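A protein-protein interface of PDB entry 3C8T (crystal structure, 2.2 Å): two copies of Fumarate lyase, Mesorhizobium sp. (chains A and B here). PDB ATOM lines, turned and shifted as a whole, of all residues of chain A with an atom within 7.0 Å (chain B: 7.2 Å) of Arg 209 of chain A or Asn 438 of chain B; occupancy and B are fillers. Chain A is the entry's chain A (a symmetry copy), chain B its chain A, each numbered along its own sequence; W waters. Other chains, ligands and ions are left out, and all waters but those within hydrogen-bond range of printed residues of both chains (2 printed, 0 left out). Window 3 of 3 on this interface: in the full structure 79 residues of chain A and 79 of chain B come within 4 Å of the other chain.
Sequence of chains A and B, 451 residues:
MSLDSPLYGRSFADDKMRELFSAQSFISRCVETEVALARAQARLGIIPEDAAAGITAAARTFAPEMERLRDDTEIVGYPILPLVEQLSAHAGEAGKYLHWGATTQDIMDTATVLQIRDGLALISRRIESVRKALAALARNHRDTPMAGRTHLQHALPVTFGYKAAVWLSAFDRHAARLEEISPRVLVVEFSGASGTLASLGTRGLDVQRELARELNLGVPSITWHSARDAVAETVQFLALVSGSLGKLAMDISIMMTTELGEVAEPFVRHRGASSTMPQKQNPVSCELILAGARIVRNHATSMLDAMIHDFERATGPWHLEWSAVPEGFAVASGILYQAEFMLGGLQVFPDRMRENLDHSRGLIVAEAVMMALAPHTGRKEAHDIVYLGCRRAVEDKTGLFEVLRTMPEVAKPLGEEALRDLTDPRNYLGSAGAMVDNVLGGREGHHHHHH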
ATOM      1  N   ALA A  40      27.110  38.848  16.481  1.00  0.00           N
ATOM      2  CA  ALA A  40      26.881  37.460  16.111  1.00  0.00           C
ATOM      3  C   ALA A  40      27.733  37.072  14.888  1.00  0.00           C
ATOM      4  O   ALA A  40      28.296  35.996  14.830  1.00  0.00           O
ATOM      5  CB  ALA A  40      25.383  37.213  15.842  1.00  0.00           C
ATOM      6  N   ARG A  43      31.666  36.798  15.756  1.00  0.00           N
ATOM      7  CA  ARG A  43      31.929  35.518  16.426  1.00  0.00           C
ATOM      8  C   ARG A  43      31.935  34.313  15.486  1.00  0.00           C
ATOM      9  O   ARG A  43      32.668  33.360  15.712  1.00  0.00           O
ATOM     10  CB  ARG A  43      30.945  35.258  17.564  1.00  0.00           C
ATOM     11  CG  ARG A  43      31.238  36.066  18.805  1.00  0.00           C
ATOM     12  CD  ARG A  43      30.633  35.433  20.044  1.00  0.00           C
ATOM     13  NE  ARG A  43      29.186  35.301  19.944  1.00  0.00           N
ATOM     14  CZ  ARG A  43      28.305  36.243  20.283  1.00  0.00           C
ATOM     15  NH1 ARG A  43      28.704  37.429  20.753  1.00  0.00           N
ATOM     16  NH2 ARG A  43      27.007  35.988  20.146  1.00  0.00           N
ATOM     17  N   LEU A  44      31.111  34.335  14.453  1.00  0.00           N
ATOM     18  CA  LEU A  44      31.058  33.214  13.512  1.00  0.00           C
ATOM     19  C   LEU A  44      32.029  33.428  12.359  1.00  0.00           C
ATOM     20  O   LEU A  44      31.990  32.700  11.372  1.00  0.00           O
ATOM     21  CB  LEU A  44      29.632  33.020  12.959  1.00  0.00           C
ATOM     22  CG  LEU A  44      28.539  32.620  13.962  1.00  0.00           C
ATOM     23  CD1 LEU A  44      27.186  33.129  13.527  1.00  0.00           C
ATOM     24  CD2 LEU A  44      28.505  31.095  14.207  1.00  0.00           C
ATOM     25  N   VAL A 188      13.472  35.439  17.871  1.00  0.00           N
ATOM     26  CA  VAL A 188      14.145  36.344  16.936  1.00  0.00           C
ATOM     27  C   VAL A 188      13.496  36.226  15.567  1.00  0.00           C
ATOM     28  O   VAL A 188      12.966  35.149  15.202  1.00  0.00           O
ATOM     29  CB  VAL A 188      15.692  35.991  16.887  1.00  0.00           C
ATOM     30  CG1 VAL A 188      16.026  34.812  15.901  1.00  0.00           C
ATOM     31  CG2 VAL A 188      16.490  37.194  16.548  1.00  0.00           C
ATOM     32  N   PHE A 190      15.230  36.540  11.945  1.00  0.00           N
ATOM     33  CA  PHE A 190      16.340  36.848  11.047  1.00  0.00           C
ATOM     34  C   PHE A 190      16.398  35.840   9.908  1.00  0.00           C
ATOM     35  O   PHE A 190      16.902  34.695  10.080  1.00  0.00           O
ATOM     36  CB  PHE A 190      17.687  36.909  11.792  1.00  0.00           C
ATOM     37  CG  PHE A 190      18.824  37.314  10.909  1.00  0.00           C
ATOM     38  CD1 PHE A 190      18.930  38.630  10.459  1.00  0.00           C
ATOM     39  CD2 PHE A 190      19.769  36.367  10.503  1.00  0.00           C
ATOM     40  CE1 PHE A 190      19.966  39.002   9.618  1.00  0.00           C
ATOM     41  CE2 PHE A 190      20.795  36.703   9.662  1.00  0.00           C
ATOM     42  CZ  PHE A 190      20.921  38.023   9.204  1.00  0.00           C
ATOM     43  N   GLY A 204      23.594  30.837   7.253  1.00  0.00           N
ATOM     44  CA  GLY A 204      22.418  31.576   7.730  1.00  0.00           C
ATOM     45  C   GLY A 204      21.846  31.158   9.074  1.00  0.00           C
ATOM     46  O   GLY A 204      21.638  31.991   9.941  1.00  0.00           O
ATOM     47  N   LEU A 205      21.604  29.865   9.251  1.00  0.00           N
ATOM     48  CA  LEU A 205      21.020  29.357  10.516  1.00  0.00           C
ATOM     49  C   LEU A 205      21.934  29.558  11.748  1.00  0.00           C
ATOM     50  O   LEU A 205      21.435  29.765  12.866  1.00  0.00           O
ATOM     51  CB  LEU A 205      20.619  27.903  10.369  1.00  0.00           C
ATOM     52  CG  LEU A 205      19.211  27.614   9.831  1.00  0.00           C
ATOM     53  CD1 LEU A 205      19.011  28.280   8.547  1.00  0.00           C
ATOM     54  CD2 LEU A 205      19.007  26.137   9.590  1.00  0.00           C
ATOM     55  N   ASP A 206      23.256  29.494  11.524  1.00  0.00           N
ATOM     56  CA  ASP A 206      24.261  29.818  12.555  1.00  0.00           C
ATOM     57  C   ASP A 206      24.111  31.262  13.038  1.00  0.00           C
ATOM     58  O   ASP A 206      24.056  31.532  14.233  1.00  0.00           O
ATOM     59  CB  ASP A 206      25.693  29.611  12.015  1.00  0.00           C
ATOM     60  CG  ASP A 206      25.941  28.206  11.558  1.00  0.00           C
ATOM     61  OD1 ASP A 206      25.428  27.270  12.226  1.00  0.00           O
ATOM     62  OD2 ASP A 206      26.635  28.029  10.521  1.00  0.00           O
ATOM     63  N   VAL A 207      24.033  32.190  12.096  1.00  0.00           N
ATOM     64  CA  VAL A 207      23.814  33.607  12.431  1.00  0.00           C
ATOM     65  C   VAL A 207      22.513  33.818  13.241  1.00  0.00           C
ATOM     66  O   VAL A 207      22.515  34.471  14.286  1.00  0.00           O
ATOM     67  CB  VAL A 207      23.795  34.454  11.163  1.00  0.00           C
ATOM     68  CG1 VAL A 207      23.521  35.942  11.485  1.00  0.00           C
ATOM     69  CG2 VAL A 207      25.111  34.275  10.410  1.00  0.00           C
ATOM     70  N   GLN A 208      21.425  33.229  12.746  1.00  0.00           N
ATOM     71  CA  GLN A 208      20.082  33.364  13.331  1.00  0.00           C
ATOM     72  C   GLN A 208      20.062  32.914  14.790  1.00  0.00           C
ATOM     73  O   GLN A 208      19.514  33.607  15.665  1.00  0.00           O
ATOM     74  CB  GLN A 208      19.051  32.556  12.497  1.00  0.00           C
ATOM     75  CG  GLN A 208      17.620  32.742  12.951  1.00  0.00           C
ATOM     76  CD  GLN A 208      16.686  31.761  12.333  1.00  0.00           C
ATOM     77  OE1 GLN A 208      16.460  30.695  12.896  1.00  0.00           O
ATOM     78  NE2 GLN A 208      16.121  32.101  11.158  1.00  0.00           N
ATOM     79  N   ARG A 209      20.654  31.752  15.038  1.00  0.00           N
ATOM     80  CA  ARG A 209      20.817  31.208  16.382  1.00  0.00           C
ATOM     81  C   ARG A 209      21.741  32.027  17.290  1.00  0.00           C
ATOM     82  O   ARG A 209      21.418  32.261  18.454  1.00  0.00           O
ATOM     83  CB  ARG A 209      21.337  29.779  16.281  1.00  0.00           C
ATOM     84  CG  ARG A 209      20.317  28.830  15.722  1.00  0.00           C
ATOM     85  CD  ARG A 209      20.984  27.563  15.241  1.00  0.00           C
ATOM     86  NE  ARG A 209      19.996  26.639  14.677  1.00  0.00           N
ATOM     87  CZ  ARG A 209      20.311  25.640  13.858  1.00  0.00           C
ATOM     88  NH1 ARG A 209      21.579  25.453  13.497  1.00  0.00           N
ATOM     89  NH2 ARG A 209      19.357  24.843  13.380  1.00  0.00           N
ATOM     90  N   GLU A 210      22.896  32.442  16.772  1.00  0.00           N
ATOM     91  CA  GLU A 210      23.771  33.345  17.517  1.00  0.00           C
ATOM     92  C   GLU A 210      23.097  34.653  17.919  1.00  0.00           C
ATOM     93  O   GLU A 210      23.286  35.155  19.033  1.00  0.00           O
ATOM     94  CB  GLU A 210      25.046  33.647  16.735  1.00  0.00           C
ATOM     95  CG  GLU A 210      26.181  32.768  17.112  1.00  0.00           C
ATOM     96  CD  GLU A 210      26.367  32.684  18.631  1.00  0.00           C
ATOM     97  OE1 GLU A 210      26.789  33.700  19.258  1.00  0.00           O
ATOM     98  OE2 GLU A 210      26.077  31.593  19.184  1.00  0.00           O
ATOM     99  N   LEU A 211      22.335  35.204  16.987  1.00  0.00           N
ATOM    100  CA  LEU A 211      21.596  36.439  17.185  1.00  0.00           C
ATOM    101  C   LEU A 211      20.520  36.303  18.269  1.00  0.00           C
ATOM    102  O   LEU A 211      20.353  37.192  19.077  1.00  0.00           O
ATOM    103  CB  LEU A 211      20.994  36.895  15.858  1.00  0.00           C
ATOM    104  CG  LEU A 211      20.113  38.143  15.857  1.00  0.00           C
ATOM    105  CD1 LEU A 211      20.934  39.328  16.235  1.00  0.00           C
ATOM    106  CD2 LEU A 211      19.525  38.342  14.475  1.00  0.00           C
ATOM    107  N   ALA A 212      19.829  35.176  18.303  1.00  0.00           N
ATOM    108  CA  ALA A 212      18.842  34.924  19.349  1.00  0.00           C
ATOM    109  C   ALA A 212      19.550  34.971  20.720  1.00  0.00           C
ATOM    110  O   ALA A 212      19.056  35.562  21.686  1.00  0.00           O
ATOM    111  CB  ALA A 212      18.184  33.587  19.118  1.00  0.00           C
ATOM    112  N   ARG A 213      20.736  34.369  20.771  1.00  0.00           N
ATOM    113  CA  ARG A 213      21.500  34.281  21.988  1.00  0.00           C
ATOM    114  C   ARG A 213      21.908  35.664  22.432  1.00  0.00           C
ATOM    115  O   ARG A 213      21.730  35.996  23.585  1.00  0.00           O
ATOM    116  CB  ARG A 213      22.697  33.358  21.787  1.00  0.00           C
ATOM    117  CG  ARG A 213      23.293  32.840  23.081  1.00  0.00           C
ATOM    118  CD  ARG A 213      24.139  31.581  22.856  1.00  0.00           C
ATOM    119  NE  ARG A 213      25.542  31.820  22.471  1.00  0.00           N
ATOM    120  CZ  ARG A 213      26.253  32.927  22.696  1.00  0.00           C
ATOM    121  NH1 ARG A 213      25.727  33.972  23.324  1.00  0.00           N
ATOM    122  NH2 ARG A 213      27.515  32.987  22.289  1.00  0.00           N
ATOM    123  N   GLU A 214      22.411  36.486  21.515  1.00  0.00           N
ATOM    124  CA  GLU A 214      22.845  37.847  21.840  1.00  0.00           C
ATOM    125  C   GLU A 214      21.727  38.695  22.436  1.00  0.00           C
ATOM    126  O   GLU A 214      21.974  39.559  23.255  1.00  0.00           O
ATOM    127  CB  GLU A 214      23.327  38.578  20.578  1.00  0.00           C
ATOM    128  CG  GLU A 214      24.799  38.577  20.320  1.00  0.00           C
ATOM    129  CD  GLU A 214      25.601  39.153  21.494  1.00  0.00           C
ATOM    130  OE1 GLU A 214      26.421  38.394  22.055  1.00  0.00           O
ATOM    131  OE2 GLU A 214      25.406  40.345  21.869  1.00  0.00           O
ATOM    132  N   LEU A 217      16.657  35.849  23.104  1.00  0.00           N
ATOM    133  CA  LEU A 217      15.350  35.440  22.580  1.00  0.00           C
ATOM    134  C   LEU A 217      15.387  33.961  22.207  1.00  0.00           C
ATOM    135  O   LEU A 217      16.485  33.382  22.049  1.00  0.00           O
ATOM    136  CB  LEU A 217      14.987  36.294  21.351  1.00  0.00           C
ATOM    137  CG  LEU A 217      14.723  37.777  21.643  1.00  0.00           C
ATOM    138  CD1 LEU A 217      14.697  38.597  20.376  1.00  0.00           C
ATOM    139  CD2 LEU A 217      13.411  38.011  22.519  1.00  0.00           C
ATOM    140  N   GLY A 218      14.223  33.327  22.045  1.00  0.00           N
ATOM    141  CA  GLY A 218      14.253  31.948  21.495  1.00  0.00           C
ATOM    142  C   GLY A 218      14.646  32.006  20.006  1.00  0.00           C
ATOM    143  O   GLY A 218      14.768  33.090  19.426  1.00  0.00           O
ATOM    144  N   VAL A 219      14.827  30.834  19.409  1.00  0.00           N
ATOM    145  CA  VAL A 219      15.048  30.643  17.993  1.00  0.00           C
ATOM    146  C   VAL A 219      13.748  30.079  17.408  1.00  0.00           C
ATOM    147  O   VAL A 219      13.238  29.083  17.908  1.00  0.00           O
ATOM    148  CB  VAL A 219      16.214  29.625  17.741  1.00  0.00           C
ATOM    149  CG1 VAL A 219      16.444  29.344  16.236  1.00  0.00           C
ATOM    150  CG2 VAL A 219      17.544  30.095  18.407  1.00  0.00           C
ATOM    151  N   PRO A 220      13.196  30.711  16.350  1.00  0.00           N
ATOM    152  CA  PRO A 220      11.987  30.171  15.719  1.00  0.00           C
ATOM    153  C   PRO A 220      12.275  28.845  15.032  1.00  0.00           C
ATOM    154  O   PRO A 220      13.437  28.563  14.646  1.00  0.00           O
ATOM    155  CB  PRO A 220      11.671  31.225  14.649  1.00  0.00           C
ATOM    156  CG  PRO A 220      13.006  31.794  14.264  1.00  0.00           C
ATOM    157  CD  PRO A 220      13.670  31.918  15.645  1.00  0.00           C
ATOM    158  N   SER A 221      11.243  28.025  14.854  1.00  0.00           N
ATOM    159  CA  SER A 221      11.415  26.783  14.098  1.00  0.00           C
ATOM    160  C   SER A 221      11.819  27.088  12.619  1.00  0.00           C
ATOM    161  O   SER A 221      12.610  26.366  12.011  1.00  0.00           O
ATOM    162  CB  SER A 221      10.134  25.975  14.124  1.00  0.00           C
ATOM    163  OG  SER A 221       9.029  26.818  13.929  1.00  0.00           O
ATOM    164  N   ILE A 222      11.243  28.174  12.089  1.00  0.00           N
ATOM    165  CA  ILE A 222      11.479  28.666  10.734  1.00  0.00           C
ATOM    166  C   ILE A 222      10.959  30.125  10.660  1.00  0.00           C
ATOM    167  O   ILE A 222      10.145  30.584  11.513  1.00  0.00           O
ATOM    168  CB  ILE A 222      10.804  27.725   9.648  1.00  0.00           C
ATOM    169  CG1 ILE A 222      11.282  28.029   8.211  1.00  0.00           C
ATOM    170  CG2 ILE A 222       9.248  27.762   9.766  1.00  0.00           C
ATOM    171  CD1 ILE A 222      10.974  26.888   7.212  1.00  0.00           C
ATOM    172  N   ASP B 172       2.369  23.001  13.936  1.00  0.00           N
ATOM    173  CA  ASP B 172       3.139  22.501  15.066  1.00  0.00           C
ATOM    174  C   ASP B 172       2.857  23.342  16.285  1.00  0.00           C
ATOM    175  O   ASP B 172       2.691  22.792  17.358  1.00  0.00           O
ATOM    176  CB  ASP B 172       4.639  22.545  14.760  1.00  0.00           C
ATOM    177  CG  ASP B 172       5.054  21.532  13.664  1.00  0.00           C
ATOM    178  OD1 ASP B 172       4.347  20.521  13.476  1.00  0.00           O
ATOM    179  OD2 ASP B 172       6.095  21.745  13.011  1.00  0.00           O
ATOM    180  N   ALA B 432      17.341  27.351   2.593  1.00  0.00           N
ATOM    181  CA  ALA B 432      16.013  26.810   2.376  1.00  0.00           C
ATOM    182  C   ALA B 432      15.930  25.339   2.816  1.00  0.00           C
ATOM    183  O   ALA B 432      15.111  24.961   3.696  1.00  0.00           O
ATOM    184  CB  ALA B 432      15.614  26.958   0.920  1.00  0.00           C
ATOM    185  N   GLY B 433      16.786  24.509   2.204  1.00  0.00           N
ATOM    186  CA  GLY B 433      16.858  23.098   2.548  1.00  0.00           C
ATOM    187  C   GLY B 433      17.073  22.866   4.039  1.00  0.00           C
ATOM    188  O   GLY B 433      16.382  22.058   4.641  1.00  0.00           O
ATOM    189  N   ALA B 434      18.053  23.543   4.633  1.00  0.00           N
ATOM    190  CA  ALA B 434      18.336  23.337   6.052  1.00  0.00           C
ATOM    191  C   ALA B 434      17.159  23.770   6.943  1.00  0.00           C
ATOM    192  O   ALA B 434      16.903  23.151   7.974  1.00  0.00           O
ATOM    193  CB  ALA B 434      19.617  24.054   6.451  1.00  0.00           C
ATOM    194  N   MET B 435      16.434  24.814   6.542  1.00  0.00           N
ATOM    195  CA  MET B 435      15.280  25.301   7.312  1.00  0.00           C
ATOM    196  C   MET B 435      14.150  24.267   7.309  1.00  0.00           C
ATOM    197  O   MET B 435      13.500  24.014   8.342  1.00  0.00           O
ATOM    198  CB  MET B 435      14.800  26.663   6.761  1.00  0.00           C
ATOM    199  CG  MET B 435      15.788  27.814   6.954  1.00  0.00           C
ATOM    200  SD  MET B 435      15.239  29.374   6.226  1.00  0.00           S
ATOM    201  CE  MET B 435      16.479  30.472   6.920  1.00  0.00           C
ATOM    202  N   VAL B 436      13.942  23.638   6.161  1.00  0.00           N
ATOM    203  CA  VAL B 436      12.983  22.555   6.030  1.00  0.00           C
ATOM    204  C   VAL B 436      13.324  21.418   6.990  1.00  0.00           C
ATOM    205  O   VAL B 436      12.421  20.917   7.681  1.00  0.00           O
ATOM    206  CB  VAL B 436      12.882  22.011   4.583  1.00  0.00           C
ATOM    207  CG1 VAL B 436      12.117  20.668   4.533  1.00  0.00           C
ATOM    208  CG2 VAL B 436      12.232  23.042   3.668  1.00  0.00           C
ATOM    209  N   ASP B 437      14.605  21.010   7.011  1.00  0.00           N
ATOM    210  CA  ASP B 437      15.079  19.913   7.874  1.00  0.00           C
ATOM    211  C   ASP B 437      14.841  20.223   9.354  1.00  0.00           C
ATOM    212  O   ASP B 437      14.433  19.371  10.134  1.00  0.00           O
ATOM    213  CB  ASP B 437      16.562  19.635   7.627  1.00  0.00           C
ATOM    214  CG  ASP B 437      16.846  19.102   6.201  1.00  0.00           C
ATOM    215  OD1 ASP B 437      15.925  18.533   5.530  1.00  0.00           O
ATOM    216  OD2 ASP B 437      18.015  19.266   5.764  1.00  0.00           O
ATOM    217  N   ASN B 438      15.091  21.467   9.725  1.00  0.00           N
ATOM    218  CA  ASN B 438      14.848  21.974  11.072  1.00  0.00           C
ATOM    219  C   ASN B 438      13.402  21.826  11.531  1.00  0.00           C
ATOM    220  O   ASN B 438      13.128  21.330  12.631  1.00  0.00           O
ATOM    221  CB  ASN B 438      15.234  23.442  11.132  1.00  0.00           C
ATOM    222  CG  ASN B 438      15.382  23.930  12.547  1.00  0.00           C
ATOM    223  OD1 ASN B 438      16.373  23.602  13.210  1.00  0.00           O
ATOM    224  ND2 ASN B 438      14.392  24.687  13.046  1.00  0.00           N
ATOM    225  N   VAL B 439      12.457  22.249  10.711  1.00  0.00           N
ATOM    226  CA  VAL B 439      11.049  22.106  11.066  1.00  0.00           C
ATOM    227  C   VAL B 439      10.623  20.615  11.108  1.00  0.00           C
ATOM    228  O   VAL B 439       9.947  20.176  12.030  1.00  0.00           O
ATOM    229  CB  VAL B 439      10.155  22.923  10.093  1.00  0.00           C
ATOM    230  CG1 VAL B 439       8.658  22.710  10.382  1.00  0.00           C
ATOM    231  CG2 VAL B 439      10.514  24.362  10.176  1.00  0.00           C
ATOM    232  N   LEU B 440      11.016  19.848  10.103  1.00  0.00           N
ATOM    233  CA  LEU B 440      10.683  18.419  10.064  1.00  0.00           C
ATOM    234  C   LEU B 440      11.246  17.669  11.299  1.00  0.00           C
ATOM    235  O   LEU B 440      10.570  16.797  11.856  1.00  0.00           O
ATOM    236  CB  LEU B 440      11.154  17.785   8.759  1.00  0.00           C
ATOM    237  CG  LEU B 440      10.374  18.203   7.497  1.00  0.00           C
ATOM    238  CD1 LEU B 440      11.001  17.566   6.251  1.00  0.00           C
ATOM    239  CD2 LEU B 440       8.906  17.773   7.568  1.00  0.00           C
ATOM    240  N   GLY B 441      12.451  18.039  11.728  1.00  0.00           N
ATOM    241  CA  GLY B 441      13.058  17.523  12.948  1.00  0.00           C
ATOM    242  C   GLY B 441      13.018  16.014  13.058  1.00  0.00           C
ATOM    243  O   GLY B 441      12.645  15.460  14.124  1.00  0.00           O
ATOM    244  N   GLY B 442      13.350  15.339  11.955  1.00  0.00           N
ATOM    245  CA  GLY B 442      13.381  13.880  11.944  1.00  0.00           C
ATOM    246  C   GLY B 442      12.016  13.230  11.770  1.00  0.00           C
ATOM    247  O   GLY B 442      11.795  12.102  12.247  1.00  0.00           O
ATOM    248  N   ARG B 443      11.093  13.937  11.115  1.00  0.00           N
ATOM    249  CA  ARG B 443       9.849  13.326  10.603  1.00  0.00           C
ATOM    250  C   ARG B 443      10.066  12.841   9.152  1.00  0.00           C
ATOM    251  O   ARG B 443      10.490  13.623   8.264  1.00  0.00           O
ATOM    252  CB  ARG B 443       8.669  14.325  10.644  1.00  0.00           C
ATOM    253  CG  ARG B 443       8.066  14.570  12.032  1.00  0.00           C
ATOM    254  CD  ARG B 443       6.963  15.647  11.930  1.00  0.00           C
ATOM    255  NE  ARG B 443       7.485  17.016  12.051  1.00  0.00           N
ATOM    256  CZ  ARG B 443       6.738  18.100  12.237  1.00  0.00           C
ATOM    257  NH1 ARG B 443       5.395  18.009  12.281  1.00  0.00           N
ATOM    258  NH2 ARG B 443       7.340  19.286  12.370  1.00  0.00           N
HETATM  259  O   HOH W   1      14.609  30.109   9.580  1.00  0.00           O
HETATM  260  O   HOH W   2      17.214  26.642  14.243  1.00  0.00           O
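Hydrophobic or aromatic side chains of chain B within 4 Å of the printed part of chain A: Ala 434, Met 435 and Val 439. Among the printed residues, 7 pairs touch across the chains. Among the printed residues, no Asp or Glu carboxylate lies within 4 Å of a Lys or Arg side-chain nitrogen of the other chain.
Among the printed residues, merely in contact across the chains: Leu 205 of chain A with Ala 434 of chain B (3.8 Å), Leu 205 of chain A with Met 435 of chain B (3.6 Å), Ser 221 of chain A with Val 439 of chain B (3.4 Å), Ile 222 of chain A with Met 435 of chain B (3.9 Å) and Ile 222 of chain A with Val 439 of chain B (3.4 Å).
The backbone carbonyl oxygen of Val 439 of chain B is in hydrogen-bond range of the guanidinium group of Arg 443 of chain B (2.8 Å).
Of the printed residues of chain B, Leu 205 of chain A touches Ala 434 and Met 435. Val 207 of chain A touches none of the printed residues of chain B. Gln 208 of chain A touches none of the printed residues of chain B. Of chain B, only Asn 438 comes within 4 Å of Arg 209 of chain A. Printed residues of chain B within 4 Å of Ser 221 of chain A: Asn 438 and Val 439. Printed residues of chain A within 4 Å of Ala 434 of chain B: Leu 205 (3.8 Å). Printed residues of chain A within 4 Å of Met 435 of chain B: Leu 205 (3.6 Å) and Ile 222 (3.9 Å). Asn 438 of chain B touches just these residues of chain A: Arg 209 and Ser 221. The nearest residue of chain A that does not touch Asn 438 of chain B is Pro 220 of chain A (4.3 Å). The nearest printed residue of chain B that does not touch Ile 222 of chain A is Val 436 of chain B (4.5 Å).
OD1 of Asn 438 of chain B sits at hydrogen-bond distance from NH2 of Arg 209 of chain A (3.2 Å). The side-chain amide nitrogen (ND2) of Asn 438 of chain B lies within hydrogen-bond range of the backbone carbonyl oxygen (O) of Ser 221 of chain A.
No position is printed for both chains. Of the 7 pairs that touch across the chains among the printed residues, none has its exchanged pair printed and touching as well.
Water W2 bridges NE of Arg 209 of chain A (2.8 Å) and OD1 of Asn 438 of chain B (3.3 Å). Water W1 bridges the side-chain amide nitrogen (NE2) of Gln 208 of chain A (3.0 Å) and the side-chain sulfur (SD) of Met 435 of chain B (3.5 Å).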
